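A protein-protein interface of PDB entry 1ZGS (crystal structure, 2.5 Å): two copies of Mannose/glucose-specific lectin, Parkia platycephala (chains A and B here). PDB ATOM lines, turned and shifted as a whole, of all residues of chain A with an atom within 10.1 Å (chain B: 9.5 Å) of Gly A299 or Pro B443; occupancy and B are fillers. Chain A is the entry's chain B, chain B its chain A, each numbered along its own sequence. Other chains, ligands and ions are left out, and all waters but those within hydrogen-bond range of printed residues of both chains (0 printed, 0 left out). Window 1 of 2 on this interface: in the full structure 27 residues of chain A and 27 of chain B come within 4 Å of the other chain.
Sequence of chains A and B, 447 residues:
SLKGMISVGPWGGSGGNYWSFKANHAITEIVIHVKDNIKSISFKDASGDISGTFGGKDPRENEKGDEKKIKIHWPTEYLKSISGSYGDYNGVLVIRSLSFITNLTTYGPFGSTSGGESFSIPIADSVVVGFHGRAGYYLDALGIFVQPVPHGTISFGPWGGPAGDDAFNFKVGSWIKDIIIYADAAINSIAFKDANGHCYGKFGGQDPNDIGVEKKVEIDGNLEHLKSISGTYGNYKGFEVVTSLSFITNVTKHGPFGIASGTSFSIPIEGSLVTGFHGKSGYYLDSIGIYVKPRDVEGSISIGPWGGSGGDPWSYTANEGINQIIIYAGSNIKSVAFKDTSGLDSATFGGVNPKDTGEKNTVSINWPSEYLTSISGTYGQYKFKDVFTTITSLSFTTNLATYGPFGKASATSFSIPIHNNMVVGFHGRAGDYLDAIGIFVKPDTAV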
ATOM      1  N   GLY A   4      14.304 -19.161  23.864  1.00  0.00           N
ATOM      2  CA  GLY A   4      14.632 -20.485  24.396  1.00  0.00           C
ATOM      3  C   GLY A   4      13.424 -21.114  25.099  1.00  0.00           C
ATOM      4  O   GLY A   4      12.700 -20.468  25.897  1.00  0.00           O
ATOM      5  N   LYS A 293      15.947 -25.127  33.152  1.00  0.00           N
ATOM      6  CA  LYS A 293      15.897 -23.838  32.489  1.00  0.00           C
ATOM      7  C   LYS A 293      16.137 -24.070  30.980  1.00  0.00           C
ATOM      8  O   LYS A 293      16.867 -24.974  30.613  1.00  0.00           O
ATOM      9  CB  LYS A 293      16.931 -22.891  33.154  1.00  0.00           C
ATOM     10  CG  LYS A 293      17.821 -22.092  32.231  1.00  0.00           C
ATOM     11  CD  LYS A 293      18.790 -21.139  32.984  1.00  0.00           C
ATOM     12  CE  LYS A 293      18.920 -19.790  32.225  1.00  0.00           C
ATOM     13  NZ  LYS A 293      20.132 -19.007  32.538  1.00  0.00           N
ATOM     14  N   PRO A 294      15.489 -23.308  30.106  1.00  0.00           N
ATOM     15  CA  PRO A 294      15.826 -23.383  28.674  1.00  0.00           C
ATOM     16  C   PRO A 294      17.255 -22.921  28.447  1.00  0.00           C
ATOM     17  O   PRO A 294      17.642 -21.886  28.966  1.00  0.00           O
ATOM     18  CB  PRO A 294      14.859 -22.390  28.028  1.00  0.00           C
ATOM     19  CG  PRO A 294      13.750 -22.261  29.024  1.00  0.00           C
ATOM     20  CD  PRO A 294      14.394 -22.360  30.368  1.00  0.00           C
ATOM     21  N   ARG A 295      18.051 -23.706  27.731  1.00  0.00           N
ATOM     22  CA  ARG A 295      19.319 -23.184  27.196  1.00  0.00           C
ATOM     23  C   ARG A 295      18.941 -22.172  26.119  1.00  0.00           C
ATOM     24  O   ARG A 295      17.879 -22.311  25.502  1.00  0.00           O
ATOM     25  CB  ARG A 295      20.177 -24.303  26.604  1.00  0.00           C
ATOM     26  CG  ARG A 295      20.000 -25.663  27.291  1.00  0.00           C
ATOM     27  CD  ARG A 295      21.262 -26.430  27.596  1.00  0.00           C
ATOM     28  NE  ARG A 295      22.228 -26.466  26.504  1.00  0.00           N
ATOM     29  CZ  ARG A 295      23.488 -26.051  26.625  1.00  0.00           C
ATOM     30  NH1 ARG A 295      23.921 -25.569  27.789  1.00  0.00           N
ATOM     31  NH2 ARG A 295      24.324 -26.131  25.596  1.00  0.00           N
ATOM     32  N   ASP A 296      19.753 -21.138  25.893  1.00  0.00           N
ATOM     33  CA  ASP A 296      19.371 -20.134  24.843  1.00  0.00           C
ATOM     34  C   ASP A 296      20.093 -20.306  23.511  1.00  0.00           C
ATOM     35  O   ASP A 296      21.140 -20.966  23.466  1.00  0.00           O
ATOM     36  CB  ASP A 296      19.419 -18.664  25.345  1.00  0.00           C
ATOM     37  CG  ASP A 296      20.378 -18.452  26.532  1.00  0.00           C
ATOM     38  OD1 ASP A 296      20.003 -18.771  27.689  1.00  0.00           O
ATOM     39  OD2 ASP A 296      21.514 -17.938  26.413  1.00  0.00           O
ATOM     40  N   GLY A 299      23.200 -16.887  22.778  1.00  0.00           N
ATOM     41  CA  GLY A 299      24.484 -16.843  23.481  1.00  0.00           C
ATOM     42  C   GLY A 299      24.695 -15.553  24.264  1.00  0.00           C
ATOM     43  O   GLY A 299      23.990 -14.536  24.061  1.00  0.00           O
ATOM     44  N   SER A 300      25.668 -15.606  25.172  1.00  0.00           N
ATOM     45  CA  SER A 300      26.005 -14.501  26.055  1.00  0.00           C
ATOM     46  C   SER A 300      27.417 -14.157  25.763  1.00  0.00           C
ATOM     47  O   SER A 300      28.238 -15.051  25.591  1.00  0.00           O
ATOM     48  CB  SER A 300      25.948 -14.947  27.508  1.00  0.00           C
ATOM     49  OG  SER A 300      24.613 -15.042  27.898  1.00  0.00           O
ATOM     50  N   ILE A 301      27.713 -12.870  25.724  1.00  0.00           N
ATOM     51  CA  ILE A 301      29.082 -12.449  25.589  1.00  0.00           C
ATOM     52  C   ILE A 301      29.642 -12.200  26.966  1.00  0.00           C
ATOM     53  O   ILE A 301      28.968 -11.659  27.834  1.00  0.00           O
ATOM     54  CB  ILE A 301      29.161 -11.201  24.704  1.00  0.00           C
ATOM     55  CG1 ILE A 301      28.865 -11.598  23.252  1.00  0.00           C
ATOM     56  CG2 ILE A 301      30.530 -10.505  24.839  1.00  0.00           C
ATOM     57  CD1 ILE A 301      28.488 -10.427  22.383  1.00  0.00           C
ATOM     58  N   SER A 302      30.885 -12.605  27.160  1.00  0.00           N
ATOM     59  CA  SER A 302      31.582 -12.436  28.417  1.00  0.00           C
ATOM     60  C   SER A 302      32.618 -11.313  28.264  1.00  0.00           C
ATOM     61  O   SER A 302      33.430 -11.343  27.324  1.00  0.00           O
ATOM     62  CB  SER A 302      32.244 -13.779  28.756  1.00  0.00           C
ATOM     63  OG  SER A 302      33.074 -13.707  29.891  1.00  0.00           O
ATOM     64  N   ILE A 303      32.566 -10.322  29.162  1.00  0.00           N
ATOM     65  CA  ILE A 303      33.501  -9.197  29.199  1.00  0.00           C
ATOM     66  C   ILE A 303      34.225  -9.184  30.530  1.00  0.00           C
ATOM     67  O   ILE A 303      33.600  -9.361  31.589  1.00  0.00           O
ATOM     68  CB  ILE A 303      32.749  -7.863  29.076  1.00  0.00           C
ATOM     69  CG1 ILE A 303      31.504  -8.008  28.197  1.00  0.00           C
ATOM     70  CG2 ILE A 303      33.694  -6.738  28.576  1.00  0.00           C
ATOM     71  CD1 ILE A 303      31.509  -7.192  26.966  1.00  0.00           C
ATOM     72  N   THR A 317      24.576 -16.479  36.563  1.00  0.00           N
ATOM     73  CA  THR A 317      23.720 -16.030  35.491  1.00  0.00           C
ATOM     74  C   THR A 317      22.300 -16.039  36.008  1.00  0.00           C
ATOM     75  O   THR A 317      21.843 -17.064  36.524  1.00  0.00           O
ATOM     76  CB  THR A 317      23.890 -16.978  34.305  1.00  0.00           C
ATOM     77  OG1 THR A 317      25.222 -16.835  33.791  1.00  0.00           O
ATOM     78  CG2 THR A 317      22.974 -16.600  33.128  1.00  0.00           C
ATOM     79  N   ASN A 420      23.591  -0.583  24.056  1.00  0.00           N
ATOM     80  CA  ASN A 420      22.661  -1.485  23.395  1.00  0.00           C
ATOM     81  C   ASN A 420      22.740  -2.909  24.001  1.00  0.00           C
ATOM     82  O   ASN A 420      22.562  -3.911  23.303  1.00  0.00           O
ATOM     83  CB  ASN A 420      22.880  -1.467  21.857  1.00  0.00           C
ATOM     84  CG  ASN A 420      21.610  -1.853  21.063  1.00  0.00           C
ATOM     85  OD1 ASN A 420      20.527  -1.262  21.253  1.00  0.00           O
ATOM     86  ND2 ASN A 420      21.734  -2.855  20.180  1.00  0.00           N
ATOM     87  N   ASN A 421      22.999  -2.986  25.306  1.00  0.00           N
ATOM     88  CA  ASN A 421      23.140  -4.272  25.973  1.00  0.00           C
ATOM     89  C   ASN A 421      22.422  -4.322  27.303  1.00  0.00           C
ATOM     90  O   ASN A 421      21.986  -3.310  27.835  1.00  0.00           O
ATOM     91  CB  ASN A 421      24.606  -4.574  26.266  1.00  0.00           C
ATOM     92  CG  ASN A 421      25.165  -3.649  27.323  1.00  0.00           C
ATOM     93  OD1 ASN A 421      25.307  -2.455  27.071  1.00  0.00           O
ATOM     94  ND2 ASN A 421      25.438  -4.177  28.527  1.00  0.00           N
ATOM     95  N   MET A 422      22.356  -5.526  27.852  1.00  0.00           N
ATOM     96  CA  MET A 422      21.952  -5.711  29.234  1.00  0.00           C
ATOM     97  C   MET A 422      22.841  -6.778  29.858  1.00  0.00           C
ATOM     98  O   MET A 422      23.219  -7.751  29.189  1.00  0.00           O
ATOM     99  CB  MET A 422      20.477  -6.107  29.320  1.00  0.00           C
ATOM    100  CG  MET A 422      20.147  -7.310  28.474  1.00  0.00           C
ATOM    101  SD  MET A 422      18.363  -7.577  28.351  1.00  0.00           S
ATOM    102  CE  MET A 422      18.300  -9.129  27.416  1.00  0.00           C
ATOM    103  N   VAL A 424      23.293  -9.819  31.953  1.00  0.00           N
ATOM    104  CA  VAL A 424      22.488 -10.953  32.366  1.00  0.00           C
ATOM    105  C   VAL A 424      23.175 -11.791  33.452  1.00  0.00           C
ATOM    106  O   VAL A 424      22.569 -12.709  33.986  1.00  0.00           O
ATOM    107  CB  VAL A 424      22.132 -11.878  31.171  1.00  0.00           C
ATOM    108  CG1 VAL A 424      21.442 -11.109  30.092  1.00  0.00           C
ATOM    109  CG2 VAL A 424      23.371 -12.569  30.640  1.00  0.00           C
ATOM    110  N   PHE A 440      28.352 -10.835  32.070  1.00  0.00           N
ATOM    111  CA  PHE A 440      27.811 -11.508  30.917  1.00  0.00           C
ATOM    112  C   PHE A 440      26.808 -10.527  30.311  1.00  0.00           C
ATOM    113  O   PHE A 440      25.969  -9.952  31.022  1.00  0.00           O
ATOM    114  CB  PHE A 440      27.158 -12.829  31.341  1.00  0.00           C
ATOM    115  CG  PHE A 440      28.157 -13.916  31.775  1.00  0.00           C
ATOM    116  CD1 PHE A 440      28.171 -14.393  33.097  1.00  0.00           C
ATOM    117  CD2 PHE A 440      29.080 -14.458  30.860  1.00  0.00           C
ATOM    118  CE1 PHE A 440      29.081 -15.423  33.487  1.00  0.00           C
ATOM    119  CE2 PHE A 440      30.009 -15.461  31.248  1.00  0.00           C
ATOM    120  CZ  PHE A 440      30.011 -15.948  32.551  1.00  0.00           C
ATOM    121  N   VAL A 441      26.907 -10.293  29.009  1.00  0.00           N
ATOM    122  CA  VAL A 441      25.957  -9.396  28.356  1.00  0.00           C
ATOM    123  C   VAL A 441      25.219 -10.006  27.183  1.00  0.00           C
ATOM    124  O   VAL A 441      25.703 -10.954  26.548  1.00  0.00           O
ATOM    125  CB  VAL A 441      26.616  -8.074  27.885  1.00  0.00           C
ATOM    126  CG1 VAL A 441      27.183  -7.312  29.065  1.00  0.00           C
ATOM    127  CG2 VAL A 441      27.672  -8.340  26.793  1.00  0.00           C
ATOM    128  N   LYS A 442      24.053  -9.425  26.911  1.00  0.00           N
ATOM    129  CA  LYS A 442      23.236  -9.700  25.728  1.00  0.00           C
ATOM    130  C   LYS A 442      22.762  -8.416  25.086  1.00  0.00           C
ATOM    131  O   LYS A 442      22.569  -7.415  25.777  1.00  0.00           O
ATOM    132  CB  LYS A 442      22.020 -10.535  26.109  1.00  0.00           C
ATOM    133  CG  LYS A 442      22.351 -11.979  26.162  1.00  0.00           C
ATOM    134  CD  LYS A 442      21.191 -12.804  26.683  1.00  0.00           C
ATOM    135  CE  LYS A 442      21.571 -14.285  26.689  1.00  0.00           C
ATOM    136  NZ  LYS A 442      20.483 -15.168  27.162  1.00  0.00           N
ATOM    137  N   PRO A 443      22.579  -8.440  23.764  1.00  0.00           N
ATOM    138  CA  PRO A 443      22.017  -7.289  23.030  1.00  0.00           C
ATOM    139  C   PRO A 443      20.656  -6.879  23.536  1.00  0.00           C
ATOM    140  O   PRO A 443      19.853  -7.760  23.813  1.00  0.00           O
ATOM    141  CB  PRO A 443      21.866  -7.814  21.600  1.00  0.00           C
ATOM    142  CG  PRO A 443      22.160  -9.266  21.650  1.00  0.00           C
ATOM    143  CD  PRO A 443      22.934  -9.556  22.870  1.00  0.00           C
ATOM    144  N   ASP A 444      20.455  -5.563  23.701  1.00  0.00           N
ATOM    145  CA  ASP A 444      19.138  -4.840  23.819  1.00  0.00           C
ATOM    146  C   ASP A 444      19.202  -3.594  24.712  1.00  0.00           C
ATOM    147  O   ASP A 444      18.854  -3.701  25.898  1.00  0.00           O
ATOM    148  CB  ASP A 444      17.998  -5.714  24.353  1.00  0.00           C
ATOM    149  CG  ASP A 444      17.063  -6.199  23.267  1.00  0.00           C
ATOM    150  OD1 ASP A 444      17.497  -6.376  22.081  1.00  0.00           O
ATOM    151  OD2 ASP A 444      15.859  -6.450  23.551  1.00  0.00           O
ATOM    152  N   ASP B 296      18.153  -7.423  11.614  1.00  0.00           N
ATOM    153  CA  ASP B 296      18.225  -8.633  12.493  1.00  0.00           C
ATOM    154  C   ASP B 296      17.405  -8.533  13.776  1.00  0.00           C
ATOM    155  O   ASP B 296      17.050  -7.422  14.183  1.00  0.00           O
ATOM    156  CB  ASP B 296      19.675  -9.115  12.767  1.00  0.00           C
ATOM    157  CG  ASP B 296      20.729  -7.993  12.642  1.00  0.00           C
ATOM    158  OD1 ASP B 296      21.145  -7.658  11.504  1.00  0.00           O
ATOM    159  OD2 ASP B 296      21.233  -7.414  13.626  1.00  0.00           O
ATOM    160  N   GLY B 299      20.131  -8.110  17.526  1.00  0.00           N
ATOM    161  CA  GLY B 299      20.821  -6.865  17.890  1.00  0.00           C
ATOM    162  C   GLY B 299      22.335  -7.019  17.975  1.00  0.00           C
ATOM    163  O   GLY B 299      22.886  -8.141  18.073  1.00  0.00           O
ATOM    164  N   SER B 300      23.016  -5.870  17.917  1.00  0.00           N
ATOM    165  CA  SER B 300      24.467  -5.788  17.991  1.00  0.00           C
ATOM    166  C   SER B 300      24.786  -4.993  19.204  1.00  0.00           C
ATOM    167  O   SER B 300      24.115  -4.019  19.487  1.00  0.00           O
ATOM    168  CB  SER B 300      25.008  -5.025  16.803  1.00  0.00           C
ATOM    169  OG  SER B 300      24.892  -5.833  15.664  1.00  0.00           O
ATOM    170  N   ILE B 301      25.814  -5.395  19.921  1.00  0.00           N
ATOM    171  CA  ILE B 301      26.275  -4.599  21.022  1.00  0.00           C
ATOM    172  C   ILE B 301      27.403  -3.734  20.529  1.00  0.00           C
ATOM    173  O   ILE B 301      28.229  -4.162  19.726  1.00  0.00           O
ATOM    174  CB  ILE B 301      26.717  -5.513  22.173  1.00  0.00           C
ATOM    175  CG1 ILE B 301      25.470  -6.118  22.827  1.00  0.00           C
ATOM    176  CG2 ILE B 301      27.588  -4.755  23.195  1.00  0.00           C
ATOM    177  CD1 ILE B 301      25.774  -7.331  23.668  1.00  0.00           C
ATOM    178  N   TYR B 371      37.643 -15.382  11.987  1.00  0.00           N
ATOM    179  CA  TYR B 371      36.782 -14.198  12.092  1.00  0.00           C
ATOM    180  C   TYR B 371      37.232 -13.241  13.196  1.00  0.00           C
ATOM    181  O   TYR B 371      37.686 -13.671  14.289  1.00  0.00           O
ATOM    182  CB  TYR B 371      35.299 -14.615  12.307  1.00  0.00           C
ATOM    183  CG  TYR B 371      35.107 -15.478  13.531  1.00  0.00           C
ATOM    184  CD1 TYR B 371      34.778 -14.909  14.750  1.00  0.00           C
ATOM    185  CD2 TYR B 371      35.311 -16.878  13.473  1.00  0.00           C
ATOM    186  CE1 TYR B 371      34.625 -15.708  15.897  1.00  0.00           C
ATOM    187  CE2 TYR B 371      35.171 -17.688  14.603  1.00  0.00           C
ATOM    188  CZ  TYR B 371      34.829 -17.096  15.815  1.00  0.00           C
ATOM    189  OH  TYR B 371      34.677 -17.865  16.952  1.00  0.00           O
ATOM    190  N   LEU B 372      37.080 -11.941  12.939  1.00  0.00           N
ATOM    191  CA  LEU B 372      37.518 -10.911  13.904  1.00  0.00           C
ATOM    192  C   LEU B 372      36.920 -11.113  15.298  1.00  0.00           C
ATOM    193  O   LEU B 372      35.779 -11.539  15.431  1.00  0.00           O
ATOM    194  CB  LEU B 372      37.197  -9.511  13.376  1.00  0.00           C
ATOM    195  CG  LEU B 372      38.012  -9.078  12.152  1.00  0.00           C
ATOM    196  CD1 LEU B 372      37.393  -7.834  11.578  1.00  0.00           C
ATOM    197  CD2 LEU B 372      39.454  -8.807  12.530  1.00  0.00           C
ATOM    198  N   THR B 373      37.686 -10.760  16.328  1.00  0.00           N
ATOM    199  CA  THR B 373      37.317 -11.029  17.720  1.00  0.00           C
ATOM    200  C   THR B 373      37.485  -9.824  18.707  1.00  0.00           C
ATOM    201  O   THR B 373      36.778  -9.716  19.742  1.00  0.00           O
ATOM    202  CB  THR B 373      38.096 -12.319  18.099  1.00  0.00           C
ATOM    203  OG1 THR B 373      37.151 -13.368  18.356  1.00  0.00           O
ATOM    204  CG2 THR B 373      38.975 -12.212  19.324  1.00  0.00           C
ATOM    205  N   ILE B 418      37.350  -9.915  26.216  1.00  0.00           N
ATOM    206  CA  ILE B 418      36.049 -10.323  25.686  1.00  0.00           C
ATOM    207  C   ILE B 418      36.118 -11.754  25.138  1.00  0.00           C
ATOM    208  O   ILE B 418      37.155 -12.186  24.663  1.00  0.00           O
ATOM    209  CB  ILE B 418      35.569  -9.341  24.578  1.00  0.00           C
ATOM    210  CG1 ILE B 418      34.048  -9.418  24.390  1.00  0.00           C
ATOM    211  CG2 ILE B 418      36.295  -9.611  23.228  1.00  0.00           C
ATOM    212  CD1 ILE B 418      33.463  -8.429  23.346  1.00  0.00           C
ATOM    213  N   HIS B 419      35.006 -12.481  25.206  1.00  0.00           N
ATOM    214  CA  HIS B 419      34.975 -13.888  24.821  1.00  0.00           C
ATOM    215  C   HIS B 419      33.601 -14.242  24.336  1.00  0.00           C
ATOM    216  O   HIS B 419      32.589 -13.629  24.734  1.00  0.00           O
ATOM    217  CB  HIS B 419      35.343 -14.815  26.008  1.00  0.00           C
ATOM    218  CG  HIS B 419      36.570 -14.374  26.750  1.00  0.00           C
ATOM    219  ND1 HIS B 419      37.838 -14.828  26.431  1.00  0.00           N
ATOM    220  CD2 HIS B 419      36.736 -13.458  27.737  1.00  0.00           C
ATOM    221  CE1 HIS B 419      38.723 -14.233  27.214  1.00  0.00           C
ATOM    222  NE2 HIS B 419      38.082 -13.388  28.005  1.00  0.00           N
ATOM    223  N   ASN B 420      33.562 -15.275  23.511  1.00  0.00           N
ATOM    224  CA  ASN B 420      32.310 -15.810  23.020  1.00  0.00           C
ATOM    225  C   ASN B 420      31.608 -14.808  22.079  1.00  0.00           C
ATOM    226  O   ASN B 420      30.371 -14.733  22.047  1.00  0.00           O
ATOM    227  CB  ASN B 420      31.414 -16.261  24.205  1.00  0.00           C
ATOM    228  CG  ASN B 420      30.422 -17.382  23.813  1.00  0.00           C
ATOM    229  OD1 ASN B 420      30.818 -18.445  23.272  1.00  0.00           O
ATOM    230  ND2 ASN B 420      29.125 -17.143  24.068  1.00  0.00           N
ATOM    231  N   ASN B 421      32.398 -14.047  21.316  1.00  0.00           N
ATOM    232  CA  ASN B 421      31.839 -13.036  20.417  1.00  0.00           C
ATOM    233  C   ASN B 421      32.475 -13.028  19.048  1.00  0.00           C
ATOM    234  O   ASN B 421      33.510 -13.640  18.816  1.00  0.00           O
ATOM    235  CB  ASN B 421      32.033 -11.630  20.984  1.00  0.00           C
ATOM    236  CG  ASN B 421      33.498 -11.219  20.986  1.00  0.00           C
ATOM    237  OD1 ASN B 421      34.287 -11.774  21.747  1.00  0.00           O
ATOM    238  ND2 ASN B 421      33.875 -10.282  20.107  1.00  0.00           N
ATOM    239  N   MET B 422      31.858 -12.272  18.153  1.00  0.00           N
ATOM    240  CA  MET B 422      32.493 -11.935  16.894  1.00  0.00           C
ATOM    241  C   MET B 422      32.205 -10.479  16.583  1.00  0.00           C
ATOM    242  O   MET B 422      31.120  -9.975  16.891  1.00  0.00           O
ATOM    243  CB  MET B 422      31.996 -12.848  15.772  1.00  0.00           C
ATOM    244  CG  MET B 422      30.491 -12.845  15.627  1.00  0.00           C
ATOM    245  SD  MET B 422      29.886 -14.208  14.588  1.00  0.00           S
ATOM    246  CE  MET B 422      28.113 -13.834  14.534  1.00  0.00           C
ATOM    247  N   VAL B 423      33.188  -9.825  15.973  1.00  0.00           N
ATOM    248  CA  VAL B 423      33.087  -8.440  15.553  1.00  0.00           C
ATOM    249  C   VAL B 423      32.368  -8.391  14.211  1.00  0.00           C
ATOM    250  O   VAL B 423      32.843  -8.895  13.199  1.00  0.00           O
ATOM    251  CB  VAL B 423      34.483  -7.800  15.467  1.00  0.00           C
ATOM    252  CG1 VAL B 423      34.435  -6.371  14.846  1.00  0.00           C
ATOM    253  CG2 VAL B 423      35.171  -7.812  16.859  1.00  0.00           C
ATOM    254  N   VAL B 424      31.203  -7.781  14.201  1.00  0.00           N
ATOM    255  CA  VAL B 424      30.454  -7.691  12.961  1.00  0.00           C
ATOM    256  C   VAL B 424      30.577  -6.316  12.313  1.00  0.00           C
ATOM    257  O   VAL B 424      30.063  -6.115  11.227  1.00  0.00           O
ATOM    258  CB  VAL B 424      28.950  -8.006  13.175  1.00  0.00           C
ATOM    259  CG1 VAL B 424      28.769  -9.385  13.767  1.00  0.00           C
ATOM    260  CG2 VAL B 424      28.291  -6.931  14.044  1.00  0.00           C
ATOM    261  N   PHE B 440      31.330  -3.310  16.806  1.00  0.00           N
ATOM    262  CA  PHE B 440      30.015  -3.888  16.991  1.00  0.00           C
ATOM    263  C   PHE B 440      30.229  -5.397  17.199  1.00  0.00           C
ATOM    264  O   PHE B 440      30.959  -6.042  16.443  1.00  0.00           O
ATOM    265  CB  PHE B 440      29.124  -3.585  15.771  1.00  0.00           C
ATOM    266  CG  PHE B 440      28.734  -2.098  15.638  1.00  0.00           C
ATOM    267  CD1 PHE B 440      29.190  -1.320  14.560  1.00  0.00           C
ATOM    268  CD2 PHE B 440      27.918  -1.485  16.604  1.00  0.00           C
ATOM    269  CE1 PHE B 440      28.813   0.047  14.442  1.00  0.00           C
ATOM    270  CE2 PHE B 440      27.564  -0.110  16.506  1.00  0.00           C
ATOM    271  CZ  PHE B 440      27.998   0.654  15.425  1.00  0.00           C
ATOM    272  N   VAL B 441      29.637  -5.962  18.242  1.00  0.00           N
ATOM    273  CA  VAL B 441      29.780  -7.399  18.454  1.00  0.00           C
ATOM    274  C   VAL B 441      28.465  -8.157  18.570  1.00  0.00           C
ATOM    275  O   VAL B 441      27.417  -7.591  18.923  1.00  0.00           O
ATOM    276  CB  VAL B 441      30.634  -7.730  19.693  1.00  0.00           C
ATOM    277  CG1 VAL B 441      32.024  -7.173  19.537  1.00  0.00           C
ATOM    278  CG2 VAL B 441      29.943  -7.233  20.985  1.00  0.00           C
ATOM    279  N   LYS B 442      28.562  -9.451  18.276  1.00  0.00           N
ATOM    280  CA  LYS B 442      27.487 -10.428  18.455  1.00  0.00           C
ATOM    281  C   LYS B 442      28.015 -11.666  19.133  1.00  0.00           C
ATOM    282  O   LYS B 442      29.188 -12.005  18.970  1.00  0.00           O
ATOM    283  CB  LYS B 442      26.873 -10.813  17.113  1.00  0.00           C
ATOM    284  CG  LYS B 442      25.832  -9.832  16.702  1.00  0.00           C
ATOM    285  CD  LYS B 442      25.326 -10.093  15.293  1.00  0.00           C
ATOM    286  CE  LYS B 442      24.251  -9.056  14.928  1.00  0.00           C
ATOM    287  NZ  LYS B 442      23.647  -9.268  13.590  1.00  0.00           N
ATOM    288  N   PRO B 443      27.158 -12.333  19.909  1.00  0.00           N
ATOM    289  CA  PRO B 443      27.504 -13.623  20.532  1.00  0.00           C
ATOM    290  C   PRO B 443      27.891 -14.666  19.511  1.00  0.00           C
ATOM    291  O   PRO B 443      27.252 -14.718  18.462  1.00  0.00           O
ATOM    292  CB  PRO B 443      26.203 -14.056  21.219  1.00  0.00           C
ATOM    293  CG  PRO B 443      25.152 -13.096  20.792  1.00  0.00           C
ATOM    294  CD  PRO B 443      25.802 -11.873  20.277  1.00  0.00           C
ATOM    295  N   ASP B 444      28.957 -15.422  19.815  1.00  0.00           N
ATOM    296  CA  ASP B 444      29.363 -16.738  19.212  1.00  0.00           C
ATOM    297  C   ASP B 444      30.887 -16.943  19.151  1.00  0.00           C
ATOM    298  O   ASP B 444      31.482 -16.734  18.086  1.00  0.00           O
ATOM    299  CB  ASP B 444      28.820 -16.955  17.799  1.00  0.00           C
ATOM    300  CG  ASP B 444      27.628 -17.879  17.760  1.00  0.00           C
ATOM    301  OD1 ASP B 444      26.827 -17.931  18.744  1.00  0.00           O
ATOM    302  OD2 ASP B 444      27.418 -18.579  16.732  1.00  0.00           O
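O of Ser A300 is in hydrogen-bond range of ND2 of Asn B420. The backbone carbonyl oxygen of Ser A302 is in hydrogen-bond range of the backbone NH of His B419 (2.9 Å). O of Ser B300 is in hydrogen-bond range of ND2 of Asn A420 (2.7 Å).
The backbone NH of Asp B444 is in hydrogen-bond range of the backbone carbonyl oxygen of Asn B420 (2.7 Å). The backbone carbonyl oxygen of Thr B373 lies within hydrogen-bond range of the side-chain amide nitrogen of Asn B421 (3.0 Å). O of Ile A301 lies within hydrogen-bond range of N of Val A441, 2.7 Å away. N of Met B422 sits at hydrogen-bond distance from O of Lys B442, at 2.8 Å. OD2 of Asp A296 lies within salt-bridge range of NZ of Lys A442 (3.0 Å). The side-chain amino group (NZ) of Lys B442 is in salt-bridge range of the side-chain carboxylate (OD2) of Asp B296, 3.0 Å away.
CG2 of Ile A301 touches CG1 of Ile B418, at 3.7 Å. Asn B421 touches Ile A301. Ile A301 touches Val B441 (CD1 to CG2, 3.8 Å). CD1 of Ile A301 touches C of Lys B442 (3.5 Å). CD1 of Ile A301 touches N of Pro B443 (3.4 Å). Ile B418 touches Ser A302. Asn A420 touches Ile B301 (O to CG1, 3.7 Å). Lys A442 touches Ile B301 (C to CD1, 3.5 Å). O of Gly B299 touches CB of Pro A443, 3.7 Å away. Ile B301 touches Pro A443 (CD1 to N, 3.4 Å).
Gly A299 touches Pro B443, and with the chains exchanged Pro A443 touches Gly B299. Ile A301 touches Asn B421, and with the chains exchanged Asn A421 touches Ile B301. Ile A301 touches Lys B442, and with the chains exchanged Lys A442 touches Ile B301. Ile A301 touches Pro B443, and with the chains exchanged Pro A443 touches Ile B301.
Gly A299 touches just one residue of chain B: Pro B443. Of chain B, only Asn B420 (2.7 Å) comes within 4 Å of Ser A300. Asp A444 touches none of the printed residues of chain B. Of the printed residues of chain A, Ser B300 touches Asn A420. Printed residues of chain A within 4 Å of Asn B421: Ile A301 (3.9 Å). Of chain A, only Gly A299 (3.6 Å) and Ile A301 (3.4 Å) come within 4 Å of Pro B443. No residue of chain A comes within 4 Å of Asp B444.
Hydrophobic or aromatic side chains of chain B within 4 Å of the printed part of chain A: Ile B301, Ile B418, His B419, Val B441 and Pro B443. Of the 20 printed residues of chain A, 9 touch a printed residue of chain B.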
